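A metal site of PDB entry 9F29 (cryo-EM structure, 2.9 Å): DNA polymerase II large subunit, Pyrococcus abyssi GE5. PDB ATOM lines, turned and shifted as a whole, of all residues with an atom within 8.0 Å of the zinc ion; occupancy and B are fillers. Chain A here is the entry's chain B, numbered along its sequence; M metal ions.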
ATOM      1  N   LYS A 705      22.527   3.170  11.535  1.00  0.00           N
ATOM      2  CA  LYS A 705      22.872   3.878  12.766  1.00  0.00           C
ATOM      3  C   LYS A 705      24.116   4.728  12.546  1.00  0.00           C
ATOM      4  O   LYS A 705      25.119   4.239  12.014  1.00  0.00           O
ATOM      5  CB  LYS A 705      23.101   2.915  13.918  1.00  0.00           C
ATOM      6  CG  LYS A 705      23.215   3.582  15.274  1.00  0.00           C
ATOM      7  CD  LYS A 705      23.262   2.559  16.389  1.00  0.00           C
ATOM      8  CE  LYS A 705      23.255   3.229  17.747  1.00  0.00           C
ATOM      9  NZ  LYS A 705      21.960   3.939  17.994  1.00  0.00           N
ATOM     10  N   CYS A 706      24.062   5.982  12.980  1.00  0.00           N
ATOM     11  CA  CYS A 706      25.189   6.900  12.839  1.00  0.00           C
ATOM     12  C   CYS A 706      26.226   6.623  13.919  1.00  0.00           C
ATOM     13  O   CYS A 706      25.872   6.523  15.096  1.00  0.00           O
ATOM     14  CB  CYS A 706      24.714   8.349  12.913  1.00  0.00           C
ATOM     15  SG  CYS A 706      26.006   9.589  12.652  1.00  0.00           S
ATOM     16  N   PRO A 707      27.504   6.487  13.562  1.00  0.00           N
ATOM     17  CA  PRO A 707      28.521   6.184  14.587  1.00  0.00           C
ATOM     18  C   PRO A 707      28.662   7.257  15.646  1.00  0.00           C
ATOM     19  O   PRO A 707      28.964   6.930  16.805  1.00  0.00           O
ATOM     20  CB  PRO A 707      29.803   6.040  13.763  1.00  0.00           C
ATOM     21  CG  PRO A 707      29.350   5.809  12.356  1.00  0.00           C
ATOM     22  CD  PRO A 707      28.073   6.558  12.212  1.00  0.00           C
ATOM     23  N   LYS A 708      28.463   8.532  15.304  1.00  0.00           N
ATOM     24  CA  LYS A 708      28.740   9.620  16.233  1.00  0.00           C
ATOM     25  C   LYS A 708      27.497  10.063  17.004  1.00  0.00           C
ATOM     26  O   LYS A 708      27.487  10.023  18.237  1.00  0.00           O
ATOM     27  CB  LYS A 708      29.340  10.800  15.462  1.00  0.00           C
ATOM     28  CG  LYS A 708      30.808  10.633  15.116  1.00  0.00           C
ATOM     29  CD  LYS A 708      31.340  11.854  14.381  1.00  0.00           C
ATOM     30  CE  LYS A 708      30.872  11.875  12.938  1.00  0.00           C
ATOM     31  NZ  LYS A 708      31.386  10.700  12.182  1.00  0.00           N
ATOM     32  N   CYS A 709      26.460  10.504  16.293  1.00  0.00           N
ATOM     33  CA  CYS A 709      25.307  11.099  16.938  1.00  0.00           C
ATOM     34  C   CYS A 709      24.257  10.095  17.385  1.00  0.00           C
ATOM     35  O   CYS A 709      23.427  10.417  18.245  1.00  0.00           O
ATOM     36  CB  CYS A 709      24.651  12.120  16.010  1.00  0.00           C
ATOM     37  SG  CYS A 709      23.492  11.417  14.822  1.00  0.00           S
ATOM     38  N   GLY A 710      24.259   8.875  16.831  1.00  0.00           N
ATOM     39  CA  GLY A 710      23.307   7.874  17.248  1.00  0.00           C
ATOM     40  C   GLY A 710      21.957   7.929  16.562  1.00  0.00           C
ATOM     41  O   GLY A 710      20.983   7.396  17.113  1.00  0.00           O
ATOM     42  N   HIS A 711      21.860   8.535  15.391  1.00  0.00           N
ATOM     43  CA  HIS A 711      20.602   8.590  14.668  1.00  0.00           C
ATOM     44  C   HIS A 711      20.257   7.226  14.082  1.00  0.00           C
ATOM     45  O   HIS A 711      21.144   6.471  13.680  1.00  0.00           O
ATOM     46  CB  HIS A 711      20.672   9.643  13.564  1.00  0.00           C
ATOM     47  CG  HIS A 711      19.349   9.931  12.919  1.00  0.00           C
ATOM     48  ND1 HIS A 711      18.227  10.250  13.643  1.00  0.00           N
ATOM     49  CD2 HIS A 711      18.976   9.970  11.616  1.00  0.00           C
ATOM     50  CE1 HIS A 711      17.216  10.466  12.826  1.00  0.00           C
ATOM     51  NE2 HIS A 711      17.641  10.300  11.586  1.00  0.00           N
ATOM     52  N   VAL A 712      18.964   6.924  14.029  1.00  0.00           N
ATOM     53  CA  VAL A 712      18.467   5.663  13.470  1.00  0.00           C
ATOM     54  C   VAL A 712      17.398   5.992  12.431  1.00  0.00           C
ATOM     55  O   VAL A 712      16.463   6.748  12.713  1.00  0.00           O
ATOM     56  CB  VAL A 712      17.898   4.738  14.558  1.00  0.00           C
ATOM     57  CG1 VAL A 712      17.348   3.477  13.944  1.00  0.00           C
ATOM     58  CG2 VAL A 712      18.967   4.409  15.583  1.00  0.00           C
ATOM     59  N   LEU A 717      22.777   8.406   4.567  1.00  0.00           N
ATOM     60  CA  LEU A 717      23.534   9.550   5.054  1.00  0.00           C
ATOM     61  C   LEU A 717      22.796  10.202   6.220  1.00  0.00           C
ATOM     62  O   LEU A 717      21.575  10.332   6.195  1.00  0.00           O
ATOM     63  CB  LEU A 717      23.771  10.567   3.941  1.00  0.00           C
ATOM     64  CG  LEU A 717      25.064  10.432   3.145  1.00  0.00           C
ATOM     65  CD1 LEU A 717      25.234  11.626   2.218  1.00  0.00           C
ATOM     66  CD2 LEU A 717      26.265  10.295   4.055  1.00  0.00           C
ATOM     67  N   CYS A 718      23.548  10.610   7.227  1.00  0.00           N
ATOM     68  CA  CYS A 718      22.964  11.185   8.435  1.00  0.00           C
ATOM     69  C   CYS A 718      22.405  12.571   8.138  1.00  0.00           C
ATOM     70  O   CYS A 718      23.144  13.443   7.679  1.00  0.00           O
ATOM     71  CB  CYS A 718      24.012  11.252   9.533  1.00  0.00           C
ATOM     72  SG  CYS A 718      23.438  11.961  11.091  1.00  0.00           S
ATOM     73  N   PRO A 719      21.112  12.815   8.386  1.00  0.00           N
ATOM     74  CA  PRO A 719      20.558  14.157   8.111  1.00  0.00           C
ATOM     75  C   PRO A 719      21.147  15.257   8.964  1.00  0.00           C
ATOM     76  O   PRO A 719      21.071  16.432   8.573  1.00  0.00           O
ATOM     77  CB  PRO A 719      19.060  13.979   8.370  1.00  0.00           C
ATOM     78  CG  PRO A 719      18.925  12.709   9.135  1.00  0.00           C
ATOM     79  CD  PRO A 719      20.074  11.841   8.762  1.00  0.00           C
ATOM     80  N   ASN A 720      21.727  14.945  10.117  1.00  0.00           N
ATOM     81  CA  ASN A 720      22.319  15.951  10.994  1.00  0.00           C
ATOM     82  C   ASN A 720      23.833  16.022  10.845  1.00  0.00           C
ATOM     83  O   ASN A 720      24.384  17.085  10.539  1.00  0.00           O
ATOM     84  CB  ASN A 720      21.940  15.661  12.453  1.00  0.00           C
ATOM     85  CG  ASN A 720      20.450  15.595  12.666  1.00  0.00           C
ATOM     86  OD1 ASN A 720      19.689  16.400  12.122  1.00  0.00           O
ATOM     87  ND2 ASN A 720      20.009  14.627  13.462  1.00  0.00           N
ATOM     88  N   CYS A 721      24.520  14.898  11.046  1.00  0.00           N
ATOM     89  CA  CYS A 721      25.979  14.887  10.951  1.00  0.00           C
ATOM     90  C   CYS A 721      26.435  15.036   9.508  1.00  0.00           C
ATOM     91  O   CYS A 721      27.318  15.851   9.205  1.00  0.00           O
ATOM     92  CB  CYS A 721      26.529  13.597  11.549  1.00  0.00           C
ATOM     93  SG  CYS A 721      26.250  13.391  13.309  1.00  0.00           S
ATOM     94  N   GLY A 722      25.828  14.270   8.603  1.00  0.00           N
ATOM     95  CA  GLY A 722      26.288  14.197   7.232  1.00  0.00           C
ATOM     96  C   GLY A 722      27.202  13.020   6.929  1.00  0.00           C
ATOM     97  O   GLY A 722      27.671  12.909   5.792  1.00  0.00           O
ATOM     98  N   THR A 723      27.448  12.149   7.894  1.00  0.00           N
ATOM     99  CA  THR A 723      28.349  11.026   7.717  1.00  0.00           C
ATOM    100  C   THR A 723      27.571   9.764   7.333  1.00  0.00           C
ATOM    101  O   THR A 723      26.340   9.710   7.413  1.00  0.00           O
ATOM    102  CB  THR A 723      29.152  10.755   8.985  1.00  0.00           C
ATOM    103  OG1 THR A 723      28.251  10.568  10.097  1.00  0.00           O
ATOM    104  CG2 THR A 723      30.058  11.932   9.292  1.00  0.00           C
ATOM    105  N   ARG A 724      28.309   8.744   6.900  1.00  0.00           N
ATOM    106  CA  ARG A 724      27.705   7.487   6.492  1.00  0.00           C
ATOM    107  C   ARG A 724      27.395   6.627   7.707  1.00  0.00           C
ATOM    108  O   ARG A 724      28.199   6.541   8.644  1.00  0.00           O
ATOM    109  CB  ARG A 724      28.623   6.742   5.531  1.00  0.00           C
ATOM    110  CG  ARG A 724      27.883   5.816   4.591  1.00  0.00           C
ATOM    111  CD  ARG A 724      28.799   5.224   3.554  1.00  0.00           C
ATOM    112  NE  ARG A 724      28.389   3.881   3.187  1.00  0.00           N
ATOM    113  CZ  ARG A 724      27.486   3.602   2.250  1.00  0.00           C
ATOM    114  NH1 ARG A 724      26.884   4.568   1.571  1.00  0.00           N
ATOM    115  NH2 ARG A 724      27.173   2.337   2.000  1.00  0.00           N
ATOM    116  N   LYS A 725      26.246   5.978   7.678  1.00  0.00           N
ATOM    117  CA  LYS A 725      25.768   5.160   8.781  1.00  0.00           C
ATOM    118  C   LYS A 725      26.037   3.679   8.514  1.00  0.00           C
ATOM    119  O   LYS A 725      26.392   3.279   7.403  1.00  0.00           O
ATOM    120  CB  LYS A 725      24.278   5.406   9.026  1.00  0.00           C
ATOM    121  CG  LYS A 725      23.915   6.870   9.182  1.00  0.00           C
ATOM    122  CD  LYS A 725      22.622   7.054   9.949  1.00  0.00           C
ATOM    123  CE  LYS A 725      21.429   7.075   9.028  1.00  0.00           C
ATOM    124  NZ  LYS A 725      20.152   7.221   9.774  1.00  0.00           N
HETATM  125 ZN    ZN M   1      24.824  11.582  12.918  1.00  0.00          ZN
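The backbone NH (N) of Cys 718 sits at hydrogen-bond distance from the backbone carbonyl oxygen (O) of Thr 723. SG of Cys 718 sits close to N of Asn 720, at 3.6 Å. The backbone NH of His 711 lies close to the side-chain sulfur of Cys 709 (3.4 Å). The side-chain sulfur of Cys 706 lies close to the side-chain hydroxyl of Thr 723 (3.5 Å). N of Cys 706 sits at hydrogen-bond distance from O of His 711, at 3.0 Å. The side-chain sulfur (SG) of Cys 706 sits close to the backbone NH (N) of Lys 708, 3.8 Å away.
The zinc ion is bound by SG of Cys 718, 2.3 Å away. The zinc ion is bound by the side-chain sulfur (SG) of Cys 709, at 2.3 Å. SG of Cys 706 binds the zinc ion (2.3 Å). SG of Cys 721 is bound to the zinc ion (2.3 Å).
Within 4 Å of the zinc ion: Cys 706, Cys 709, Cys 718 and Cys 721. The nearest printed residue that does not touch the zinc ion is Thr 723 (4.6 Å).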
